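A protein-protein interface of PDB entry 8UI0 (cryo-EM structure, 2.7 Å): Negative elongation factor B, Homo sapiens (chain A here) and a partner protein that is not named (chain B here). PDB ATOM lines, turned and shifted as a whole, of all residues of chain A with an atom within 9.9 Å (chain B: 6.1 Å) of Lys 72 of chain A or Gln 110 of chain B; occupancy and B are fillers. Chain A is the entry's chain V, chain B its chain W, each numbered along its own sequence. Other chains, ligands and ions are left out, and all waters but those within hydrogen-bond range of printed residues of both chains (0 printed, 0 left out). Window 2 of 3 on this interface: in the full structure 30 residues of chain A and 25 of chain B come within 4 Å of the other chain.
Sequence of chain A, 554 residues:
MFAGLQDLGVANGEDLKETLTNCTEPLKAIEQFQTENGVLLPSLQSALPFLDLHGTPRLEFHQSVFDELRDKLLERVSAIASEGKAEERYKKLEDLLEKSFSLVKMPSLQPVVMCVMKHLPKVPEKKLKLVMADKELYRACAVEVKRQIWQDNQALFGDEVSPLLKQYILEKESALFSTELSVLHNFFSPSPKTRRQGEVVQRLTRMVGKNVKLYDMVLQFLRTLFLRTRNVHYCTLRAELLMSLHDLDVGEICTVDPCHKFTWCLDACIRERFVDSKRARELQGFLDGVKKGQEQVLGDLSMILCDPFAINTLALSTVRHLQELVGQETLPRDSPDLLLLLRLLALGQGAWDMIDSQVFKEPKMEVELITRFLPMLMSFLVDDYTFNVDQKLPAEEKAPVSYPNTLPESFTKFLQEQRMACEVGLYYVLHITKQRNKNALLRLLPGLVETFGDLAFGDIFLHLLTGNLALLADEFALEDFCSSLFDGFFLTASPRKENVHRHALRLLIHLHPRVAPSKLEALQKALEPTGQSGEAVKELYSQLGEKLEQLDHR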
ATOM      1  N   LEU A  41     -29.188 -15.816 -10.390  1.00  0.00           N
ATOM      2  CA  LEU A  41     -29.052 -16.478 -11.677  1.00  0.00           C
ATOM      3  C   LEU A  41     -30.234 -16.090 -12.552  1.00  0.00           C
ATOM      4  O   LEU A  41     -31.333 -15.865 -12.034  1.00  0.00           O
ATOM      5  CB  LEU A  41     -28.994 -18.007 -11.533  1.00  0.00           C
ATOM      6  CG  LEU A  41     -27.986 -18.564 -10.525  1.00  0.00           C
ATOM      7  CD1 LEU A  41     -28.693 -19.053  -9.274  1.00  0.00           C
ATOM      8  CD2 LEU A  41     -27.165 -19.686 -11.143  1.00  0.00           C
ATOM      9  N   SER A  64     -32.318 -26.904   0.219  1.00  0.00           N
ATOM     10  CA  SER A  64     -31.628 -28.043  -0.387  1.00  0.00           C
ATOM     11  C   SER A  64     -30.254 -27.634  -0.915  1.00  0.00           C
ATOM     12  O   SER A  64     -29.229 -28.259  -0.588  1.00  0.00           O
ATOM     13  CB  SER A  64     -32.483 -28.636  -1.508  1.00  0.00           C
ATOM     14  OG  SER A  64     -32.496 -27.790  -2.643  1.00  0.00           O
ATOM     15  N   VAL A  65     -30.207 -26.561  -1.711  1.00  0.00           N
ATOM     16  CA  VAL A  65     -28.919 -26.121  -2.235  1.00  0.00           C
ATOM     17  C   VAL A  65     -28.041 -25.566  -1.116  1.00  0.00           C
ATOM     18  O   VAL A  65     -26.819 -25.609  -1.215  1.00  0.00           O
ATOM     19  CB  VAL A  65     -29.095 -25.104  -3.385  1.00  0.00           C
ATOM     20  CG1 VAL A  65     -29.988 -25.679  -4.483  1.00  0.00           C
ATOM     21  CG2 VAL A  65     -29.637 -23.783  -2.886  1.00  0.00           C
ATOM     22  N   PHE A  66     -28.632 -25.059  -0.033  1.00  0.00           N
ATOM     23  CA  PHE A  66     -27.845 -24.601   1.112  1.00  0.00           C
ATOM     24  C   PHE A  66     -27.049 -25.751   1.713  1.00  0.00           C
ATOM     25  O   PHE A  66     -25.830 -25.646   1.917  1.00  0.00           O
ATOM     26  CB  PHE A  66     -28.785 -23.957   2.146  1.00  0.00           C
ATOM     27  CG  PHE A  66     -28.332 -24.081   3.581  1.00  0.00           C
ATOM     28  CD1 PHE A  66     -27.479 -23.146   4.136  1.00  0.00           C
ATOM     29  CD2 PHE A  66     -28.823 -25.094   4.397  1.00  0.00           C
ATOM     30  CE1 PHE A  66     -27.074 -23.248   5.454  1.00  0.00           C
ATOM     31  CE2 PHE A  66     -28.422 -25.200   5.714  1.00  0.00           C
ATOM     32  CZ  PHE A  66     -27.550 -24.272   6.244  1.00  0.00           C
ATOM     33  N   ASP A  67     -27.726 -26.874   1.970  1.00  0.00           N
ATOM     34  CA  ASP A  67     -27.031 -28.049   2.489  1.00  0.00           C
ATOM     35  C   ASP A  67     -25.953 -28.517   1.516  1.00  0.00           C
ATOM     36  O   ASP A  67     -24.792 -28.723   1.905  1.00  0.00           O
ATOM     37  CB  ASP A  67     -28.032 -29.170   2.769  1.00  0.00           C
ATOM     38  CG  ASP A  67     -27.563 -30.113   3.859  1.00  0.00           C
ATOM     39  OD1 ASP A  67     -26.334 -30.290   4.006  1.00  0.00           O
ATOM     40  OD2 ASP A  67     -28.420 -30.674   4.573  1.00  0.00           O
ATOM     41  N   GLU A  68     -26.312 -28.628   0.228  1.00  0.00           N
ATOM     42  CA  GLU A  68     -25.368 -29.118  -0.780  1.00  0.00           C
ATOM     43  C   GLU A  68     -24.135 -28.221  -0.880  1.00  0.00           C
ATOM     44  O   GLU A  68     -22.988 -28.698  -0.847  1.00  0.00           O
ATOM     45  CB  GLU A  68     -26.080 -29.206  -2.133  1.00  0.00           C
ATOM     46  CG  GLU A  68     -25.300 -29.909  -3.243  1.00  0.00           C
ATOM     47  CD  GLU A  68     -25.191 -31.406  -3.033  1.00  0.00           C
ATOM     48  OE1 GLU A  68     -26.190 -32.027  -2.614  1.00  0.00           O
ATOM     49  OE2 GLU A  68     -24.103 -31.965  -3.289  1.00  0.00           O
ATOM     50  N   LEU A  69     -24.351 -26.912  -0.970  1.00  0.00           N
ATOM     51  CA  LEU A  69     -23.264 -25.990  -1.249  1.00  0.00           C
ATOM     52  C   LEU A  69     -22.377 -25.766  -0.032  1.00  0.00           C
ATOM     53  O   LEU A  69     -21.165 -25.602  -0.203  1.00  0.00           O
ATOM     54  CB  LEU A  69     -23.822 -24.663  -1.778  1.00  0.00           C
ATOM     55  CG  LEU A  69     -24.668 -24.725  -3.067  1.00  0.00           C
ATOM     56  CD1 LEU A  69     -25.575 -23.506  -3.176  1.00  0.00           C
ATOM     57  CD2 LEU A  69     -23.827 -24.847  -4.313  1.00  0.00           C
ATOM     58  N   ARG A  70     -22.914 -25.788   1.201  1.00  0.00           N
ATOM     59  CA  ARG A  70     -21.996 -25.703   2.338  1.00  0.00           C
ATOM     60  C   ARG A  70     -21.241 -27.009   2.542  1.00  0.00           C
ATOM     61  O   ARG A  70     -20.102 -26.984   3.027  1.00  0.00           O
ATOM     62  CB  ARG A  70     -22.703 -25.322   3.637  1.00  0.00           C
ATOM     63  CG  ARG A  70     -21.704 -25.094   4.783  1.00  0.00           C
ATOM     64  CD  ARG A  70     -22.309 -24.351   5.959  1.00  0.00           C
ATOM     65  NE  ARG A  70     -23.564 -24.948   6.400  1.00  0.00           N
ATOM     66  CZ  ARG A  70     -23.668 -26.106   7.043  1.00  0.00           C
ATOM     67  NH1 ARG A  70     -22.604 -26.828   7.366  1.00  0.00           N
ATOM     68  NH2 ARG A  70     -24.876 -26.550   7.377  1.00  0.00           N
ATOM     69  N   ASP A  71     -21.843 -28.154   2.191  1.00  0.00           N
ATOM     70  CA  ASP A  71     -21.071 -29.393   2.205  1.00  0.00           C
ATOM     71  C   ASP A  71     -19.885 -29.297   1.255  1.00  0.00           C
ATOM     72  O   ASP A  71     -18.751 -29.644   1.619  1.00  0.00           O
ATOM     73  CB  ASP A  71     -21.963 -30.578   1.830  1.00  0.00           C
ATOM     74  CG  ASP A  71     -22.980 -30.908   2.906  1.00  0.00           C
ATOM     75  OD1 ASP A  71     -23.015 -30.205   3.938  1.00  0.00           O
ATOM     76  OD2 ASP A  71     -23.748 -31.875   2.718  1.00  0.00           O
ATOM     77  N   LYS A  72     -20.116 -28.779   0.046  1.00  0.00           N
ATOM     78  CA  LYS A  72     -19.005 -28.611  -0.885  1.00  0.00           C
ATOM     79  C   LYS A  72     -18.020 -27.543  -0.415  1.00  0.00           C
ATOM     80  O   LYS A  72     -16.818 -27.663  -0.675  1.00  0.00           O
ATOM     81  CB  LYS A  72     -19.527 -28.287  -2.283  1.00  0.00           C
ATOM     82  CG  LYS A  72     -20.018 -29.525  -3.010  1.00  0.00           C
ATOM     83  CD  LYS A  72     -20.691 -29.204  -4.332  1.00  0.00           C
ATOM     84  CE  LYS A  72     -21.328 -30.449  -4.935  1.00  0.00           C
ATOM     85  NZ  LYS A  72     -20.344 -31.551  -5.150  1.00  0.00           N
ATOM     86  N   LEU A  73     -18.491 -26.504   0.280  1.00  0.00           N
ATOM     87  CA  LEU A  73     -17.573 -25.488   0.791  1.00  0.00           C
ATOM     88  C   LEU A  73     -16.652 -26.063   1.861  1.00  0.00           C
ATOM     89  O   LEU A  73     -15.459 -25.749   1.889  1.00  0.00           O
ATOM     90  CB  LEU A  73     -18.354 -24.289   1.338  1.00  0.00           C
ATOM     91  CG  LEU A  73     -17.551 -23.119   1.930  1.00  0.00           C
ATOM     92  CD1 LEU A  73     -16.531 -22.562   0.939  1.00  0.00           C
ATOM     93  CD2 LEU A  73     -18.488 -22.013   2.393  1.00  0.00           C
ATOM     94  N   LEU A  74     -17.185 -26.897   2.757  1.00  0.00           N
ATOM     95  CA  LEU A  74     -16.331 -27.551   3.748  1.00  0.00           C
ATOM     96  C   LEU A  74     -15.355 -28.517   3.082  1.00  0.00           C
ATOM     97  O   LEU A  74     -14.171 -28.584   3.461  1.00  0.00           O
ATOM     98  CB  LEU A  74     -17.194 -28.280   4.778  1.00  0.00           C
ATOM     99  CG  LEU A  74     -17.702 -27.384   5.910  1.00  0.00           C
ATOM    100  CD1 LEU A  74     -19.086 -27.814   6.377  1.00  0.00           C
ATOM    101  CD2 LEU A  74     -16.723 -27.365   7.079  1.00  0.00           C
ATOM    102  N   GLU A  75     -15.839 -29.268   2.083  1.00  0.00           N
ATOM    103  CA  GLU A  75     -14.968 -30.152   1.313  1.00  0.00           C
ATOM    104  C   GLU A  75     -13.819 -29.376   0.686  1.00  0.00           C
ATOM    105  O   GLU A  75     -12.663 -29.812   0.726  1.00  0.00           O
ATOM    106  CB  GLU A  75     -15.773 -30.855   0.222  1.00  0.00           C
ATOM    107  CG  GLU A  75     -16.727 -31.922   0.723  1.00  0.00           C
ATOM    108  CD  GLU A  75     -17.809 -32.245  -0.289  1.00  0.00           C
ATOM    109  OE1 GLU A  75     -17.487 -32.348  -1.492  1.00  0.00           O
ATOM    110  OE2 GLU A  75     -18.981 -32.390   0.116  1.00  0.00           O
ATOM    111  N   ARG A  76     -14.115 -28.203   0.131  1.00  0.00           N
ATOM    112  CA  ARG A  76     -13.089 -27.393  -0.504  1.00  0.00           C
ATOM    113  C   ARG A  76     -12.195 -26.679   0.500  1.00  0.00           C
ATOM    114  O   ARG A  76     -11.049 -26.380   0.167  1.00  0.00           O
ATOM    115  CB  ARG A  76     -13.742 -26.382  -1.446  1.00  0.00           C
ATOM    116  CG  ARG A  76     -12.777 -25.521  -2.244  1.00  0.00           C
ATOM    117  CD  ARG A  76     -11.798 -26.305  -3.105  1.00  0.00           C
ATOM    118  NE  ARG A  76     -11.237 -25.482  -4.173  1.00  0.00           N
ATOM    119  CZ  ARG A  76     -10.136 -25.761  -4.864  1.00  0.00           C
ATOM    120  NH1 ARG A  76      -9.417 -26.849  -4.629  1.00  0.00           N
ATOM    121  NH2 ARG A  76      -9.741 -24.919  -5.815  1.00  0.00           N
ATOM    122  N   VAL A  77     -12.679 -26.394   1.709  1.00  0.00           N
ATOM    123  CA  VAL A  77     -11.787 -25.910   2.761  1.00  0.00           C
ATOM    124  C   VAL A  77     -10.725 -26.960   3.053  1.00  0.00           C
ATOM    125  O   VAL A  77      -9.521 -26.665   3.090  1.00  0.00           O
ATOM    126  CB  VAL A  77     -12.596 -25.537   4.021  1.00  0.00           C
ATOM    127  CG1 VAL A  77     -11.721 -25.523   5.291  1.00  0.00           C
ATOM    128  CG2 VAL A  77     -13.256 -24.181   3.833  1.00  0.00           C
ATOM    129  N   SER A  78     -11.157 -28.213   3.227  1.00  0.00           N
ATOM    130  CA  SER A  78     -10.197 -29.298   3.429  1.00  0.00           C
ATOM    131  C   SER A  78      -9.283 -29.460   2.215  1.00  0.00           C
ATOM    132  O   SER A  78      -8.078 -29.722   2.357  1.00  0.00           O
ATOM    133  CB  SER A  78     -10.938 -30.601   3.725  1.00  0.00           C
ATOM    134  OG  SER A  78     -11.722 -30.482   4.900  1.00  0.00           O
ATOM    135  N   ALA A  79      -9.835 -29.296   1.013  1.00  0.00           N
ATOM    136  CA  ALA A  79      -9.027 -29.437  -0.194  1.00  0.00           C
ATOM    137  C   ALA A  79      -7.948 -28.361  -0.267  1.00  0.00           C
ATOM    138  O   ALA A  79      -6.764 -28.678  -0.393  1.00  0.00           O
ATOM    139  CB  ALA A  79      -9.922 -29.394  -1.430  1.00  0.00           C
ATOM    140  N   ILE A  80      -8.329 -27.084  -0.136  1.00  0.00           N
ATOM    141  CA  ILE A  80      -7.355 -25.992  -0.211  1.00  0.00           C
ATOM    142  C   ILE A  80      -6.351 -26.103   0.928  1.00  0.00           C
ATOM    143  O   ILE A  80      -5.208 -25.645   0.800  1.00  0.00           O
ATOM    144  CB  ILE A  80      -8.065 -24.611  -0.233  1.00  0.00           C
ATOM    145  CG1 ILE A  80      -8.979 -24.506  -1.465  1.00  0.00           C
ATOM    146  CG2 ILE A  80      -7.044 -23.429  -0.293  1.00  0.00           C
ATOM    147  CD1 ILE A  80      -9.821 -23.237  -1.561  1.00  0.00           C
ATOM    148  N   GLU A  83      -4.645 -28.912  -1.059  1.00  0.00           N
ATOM    149  CA  GLU A  83      -4.574 -28.762  -2.512  1.00  0.00           C
ATOM    150  C   GLU A  83      -4.129 -27.349  -2.867  1.00  0.00           C
ATOM    151  O   GLU A  83      -4.341 -26.402  -2.103  1.00  0.00           O
ATOM    152  CB  GLU A  83      -5.938 -29.067  -3.178  1.00  0.00           C
ATOM    153  CG  GLU A  83      -5.956 -29.041  -4.700  1.00  0.00           C
ATOM    154  CD  GLU A  83      -7.285 -29.495  -5.272  1.00  0.00           C
ATOM    155  OE1 GLU A  83      -8.226 -29.727  -4.485  1.00  0.00           O
ATOM    156  OE2 GLU A  83      -7.391 -29.614  -6.511  1.00  0.00           O
ATOM    157  N   LEU A  96     -10.767 -16.252   2.498  1.00  0.00           N
ATOM    158  CA  LEU A  96     -12.066 -16.831   2.825  1.00  0.00           C
ATOM    159  C   LEU A  96     -12.361 -16.722   4.316  1.00  0.00           C
ATOM    160  O   LEU A  96     -13.523 -16.593   4.712  1.00  0.00           O
ATOM    161  CB  LEU A  96     -12.099 -18.293   2.369  1.00  0.00           C
ATOM    162  CG  LEU A  96     -13.260 -19.202   2.785  1.00  0.00           C
ATOM    163  CD1 LEU A  96     -14.594 -18.622   2.356  1.00  0.00           C
ATOM    164  CD2 LEU A  96     -13.064 -20.585   2.187  1.00  0.00           C
ATOM    165  N   VAL A 112     -16.991 -24.105   9.445  1.00  0.00           N
ATOM    166  CA  VAL A 112     -16.169 -23.898   8.254  1.00  0.00           C
ATOM    167  C   VAL A 112     -14.920 -23.110   8.625  1.00  0.00           C
ATOM    168  O   VAL A 112     -13.787 -23.530   8.350  1.00  0.00           O
ATOM    169  CB  VAL A 112     -16.980 -23.181   7.154  1.00  0.00           C
ATOM    170  CG1 VAL A 112     -16.191 -23.120   5.841  1.00  0.00           C
ATOM    171  CG2 VAL A 112     -18.344 -23.851   6.943  1.00  0.00           C
ATOM    172  N   LEU B 101     -18.738 -20.793  -3.130  1.00  0.00           N
ATOM    173  CA  LEU B 101     -18.281 -21.863  -4.014  1.00  0.00           C
ATOM    174  C   LEU B 101     -17.728 -21.290  -5.312  1.00  0.00           C
ATOM    175  O   LEU B 101     -16.762 -21.822  -5.869  1.00  0.00           O
ATOM    176  CB  LEU B 101     -19.406 -22.858  -4.313  1.00  0.00           C
ATOM    177  CG  LEU B 101     -19.775 -23.997  -3.344  1.00  0.00           C
ATOM    178  CD1 LEU B 101     -20.519 -25.067  -4.117  1.00  0.00           C
ATOM    179  CD2 LEU B 101     -18.598 -24.639  -2.619  1.00  0.00           C
ATOM    180  N   VAL B 106     -14.063 -23.483  -8.184  1.00  0.00           N
ATOM    181  CA  VAL B 106     -14.786 -24.627  -8.723  1.00  0.00           C
ATOM    182  C   VAL B 106     -15.763 -24.129  -9.784  1.00  0.00           C
ATOM    183  O   VAL B 106     -16.280 -23.006  -9.708  1.00  0.00           O
ATOM    184  CB  VAL B 106     -15.506 -25.391  -7.592  1.00  0.00           C
ATOM    185  CG1 VAL B 106     -16.388 -26.515  -8.145  1.00  0.00           C
ATOM    186  CG2 VAL B 106     -14.491 -25.949  -6.593  1.00  0.00           C
ATOM    187  N   GLU B 107     -16.004 -24.963 -10.793  1.00  0.00           N
ATOM    188  CA  GLU B 107     -16.810 -24.550 -11.933  1.00  0.00           C
ATOM    189  C   GLU B 107     -18.253 -24.280 -11.493  1.00  0.00           C
ATOM    190  O   GLU B 107     -18.866 -25.150 -10.857  1.00  0.00           O
ATOM    191  CB  GLU B 107     -16.791 -25.637 -13.006  1.00  0.00           C
ATOM    192  CG  GLU B 107     -17.134 -25.140 -14.403  1.00  0.00           C
ATOM    193  CD  GLU B 107     -17.377 -26.267 -15.392  1.00  0.00           C
ATOM    194  OE1 GLU B 107     -17.280 -27.449 -14.996  1.00  0.00           O
ATOM    195  OE2 GLU B 107     -17.667 -25.970 -16.570  1.00  0.00           O
ATOM    196  N   PRO B 108     -18.836 -23.106 -11.794  1.00  0.00           N
ATOM    197  CA  PRO B 108     -20.257 -22.910 -11.455  1.00  0.00           C
ATOM    198  C   PRO B 108     -21.203 -23.797 -12.248  1.00  0.00           C
ATOM    199  O   PRO B 108     -22.353 -23.983 -11.825  1.00  0.00           O
ATOM    200  CB  PRO B 108     -20.498 -21.426 -11.766  1.00  0.00           C
ATOM    201  CG  PRO B 108     -19.473 -21.079 -12.761  1.00  0.00           C
ATOM    202  CD  PRO B 108     -18.267 -21.878 -12.388  1.00  0.00           C
ATOM    203  N   VAL B 109     -20.763 -24.347 -13.381  1.00  0.00           N
ATOM    204  CA  VAL B 109     -21.628 -25.245 -14.141  1.00  0.00           C
ATOM    205  C   VAL B 109     -21.864 -26.532 -13.362  1.00  0.00           C
ATOM    206  O   VAL B 109     -22.892 -27.192 -13.544  1.00  0.00           O
ATOM    207  CB  VAL B 109     -21.050 -25.523 -15.543  1.00  0.00           C
ATOM    208  CG1 VAL B 109     -22.079 -26.253 -16.411  1.00  0.00           C
ATOM    209  CG2 VAL B 109     -20.623 -24.217 -16.226  1.00  0.00           C
ATOM    210  N   GLN B 110     -20.931 -26.913 -12.483  1.00  0.00           N
ATOM    211  CA  GLN B 110     -21.193 -28.010 -11.557  1.00  0.00           C
ATOM    212  C   GLN B 110     -22.386 -27.690 -10.663  1.00  0.00           C
ATOM    213  O   GLN B 110     -23.258 -28.540 -10.447  1.00  0.00           O
ATOM    214  CB  GLN B 110     -19.945 -28.289 -10.717  1.00  0.00           C
ATOM    215  CG  GLN B 110     -20.081 -29.416  -9.694  1.00  0.00           C
ATOM    216  CD  GLN B 110     -18.777 -29.711  -8.979  1.00  0.00           C
ATOM    217  OE1 GLN B 110     -17.721 -29.199  -9.353  1.00  0.00           O
ATOM    218  NE2 GLN B 110     -18.844 -30.535  -7.940  1.00  0.00           N
ATOM    219  N   VAL B 111     -22.445 -26.458 -10.150  1.00  0.00           N
ATOM    220  CA  VAL B 111     -23.581 -26.044  -9.331  1.00  0.00           C
ATOM    221  C   VAL B 111     -24.857 -26.045 -10.162  1.00  0.00           C
ATOM    222  O   VAL B 111     -25.924 -26.450  -9.684  1.00  0.00           O
ATOM    223  CB  VAL B 111     -23.319 -24.663  -8.699  1.00  0.00           C
ATOM    224  CG1 VAL B 111     -24.538 -24.204  -7.898  1.00  0.00           C
ATOM    225  CG2 VAL B 111     -22.070 -24.702  -7.814  1.00  0.00           C
ATOM    226  N   GLN B 112     -24.773 -25.581 -11.412  1.00  0.00           N
ATOM    227  CA  GLN B 112     -25.948 -25.575 -12.283  1.00  0.00           C
ATOM    228  C   GLN B 112     -26.469 -26.988 -12.511  1.00  0.00           C
ATOM    229  O   GLN B 112     -27.676 -27.240 -12.414  1.00  0.00           O
ATOM    230  CB  GLN B 112     -25.611 -24.915 -13.621  1.00  0.00           C
ATOM    231  CG  GLN B 112     -25.476 -23.400 -13.575  1.00  0.00           C
ATOM    232  CD  GLN B 112     -26.249 -22.715 -14.689  1.00  0.00           C
ATOM    233  OE1 GLN B 112     -27.449 -22.939 -14.853  1.00  0.00           O
ATOM    234  NE2 GLN B 112     -25.563 -21.883 -15.463  1.00  0.00           N
ATOM    235  N   GLU B 113     -25.566 -27.928 -12.801  1.00  0.00           N
ATOM    236  CA  GLU B 113     -25.971 -29.314 -13.003  1.00  0.00           C
ATOM    237  C   GLU B 113     -26.568 -29.904 -11.734  1.00  0.00           C
ATOM    238  O   GLU B 113     -27.568 -30.627 -11.794  1.00  0.00           O
ATOM    239  CB  GLU B 113     -24.778 -30.154 -13.466  1.00  0.00           C
ATOM    240  CG  GLU B 113     -24.334 -29.885 -14.899  1.00  0.00           C
ATOM    241  CD  GLU B 113     -23.633 -31.074 -15.529  1.00  0.00           C
ATOM    242  OE1 GLU B 113     -24.208 -32.184 -15.521  1.00  0.00           O
ATOM    243  OE2 GLU B 113     -22.504 -30.900 -16.033  1.00  0.00           O
ATOM    244  N   THR B 114     -25.974 -29.606 -10.575  1.00  0.00           N
ATOM    245  CA  THR B 114     -26.485 -30.149  -9.320  1.00  0.00           C
ATOM    246  C   THR B 114     -27.892 -29.633  -9.030  1.00  0.00           C
ATOM    247  O   THR B 114     -28.792 -30.409  -8.681  1.00  0.00           O
ATOM    248  CB  THR B 114     -25.536 -29.795  -8.174  1.00  0.00           C
ATOM    249  OG1 THR B 114     -24.227 -30.306  -8.459  1.00  0.00           O
ATOM    250  CG2 THR B 114     -26.028 -30.387  -6.863  1.00  0.00           C
ATOM    251  N   VAL B 115     -28.103 -28.323  -9.185  1.00  0.00           N
ATOM    252  CA  VAL B 115     -29.415 -27.741  -8.920  1.00  0.00           C
ATOM    253  C   VAL B 115     -30.447 -28.266  -9.911  1.00  0.00           C
ATOM    254  O   VAL B 115     -31.580 -28.595  -9.531  1.00  0.00           O
ATOM    255  CB  VAL B 115     -29.332 -26.202  -8.946  1.00  0.00           C
ATOM    256  CG1 VAL B 115     -30.730 -25.584  -8.865  1.00  0.00           C
ATOM    257  CG2 VAL B 115     -28.465 -25.703  -7.800  1.00  0.00           C
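The side-chain amide nitrogen (NE2) of Gln 110 of chain B lies close to the side-chain amino group (NZ) of Lys 72 of chain A.
Printed residues of chain B within 4 Å of Leu 69 of chain A: Leu 101 (3.3 Å) and Val 111 (3.7 Å). Lys 72 of chain A touches just these residues of chain B: Leu 101 (3.7 Å) and Gln 110 (3.3 Å). Val 77 of chain A touches none of the printed residues of chain B. Printed residues of chain A within 4 Å of Leu 101 of chain B: Leu 69, Lys 72 and Leu 73. No residue of chain A comes within 4 Å of Val 109 of chain B. Glu 113 of chain B touches none of the printed residues of chain A. The nearest residue of chain A that does not touch Gln 110 of chain B is Glu 75 of chain A (6.8 Å). The nearest printed residue of chain A that does not touch Val 115 of chain B is Leu 69 of chain A (5.9 Å).
Val 65 of chain A touches Val 115 of chain B (CG1 to CG2, 3.7 Å). CG of Glu 68 of chain A touches CG2 of Thr 114 of chain B, 3.7 Å away. CD1 of Leu 101 of chain B touches CD2 of Leu 69 of chain A (3.3 Å). CG1 of Val 111 of chain B touches CD2 of Leu 69 of chain A (3.7 Å). Lys 72 of chain A touches Leu 101 of chain B (C to CD2, 3.7 Å). N of Leu 73 of chain A touches CD2 of Leu 101 of chain B (3.4 Å).
Of the 21 printed residues of chain A, 5 touch a printed residue of chain B. Printed residues of chain A that touch a printed residue of chain B: Val 65, Glu 68, Leu 69, Lys 72 and Leu 73. Hydrophobic or aromatic side chains of chain A that line the printed part of chain B: Val 65, Leu 69 and Leu 73. Hydrophobic or aromatic side chains of chain B within 4 Å of the printed part of chain A: Leu 101, Val 111 and Val 115. Along chain B the printed residues that touch a printed residue of chain A span positions 101 to 115. Among the printed residues, 7 pairs touch across the chains. Among the printed residues, no Asp or Glu carboxylate lies within 4 Å of a Lys or Arg side-chain nitrogen of the other chain.
O of Gln 110 of chain B is in hydrogen-bond range of OG1 of Thr 114 of chain B (2.8 Å).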
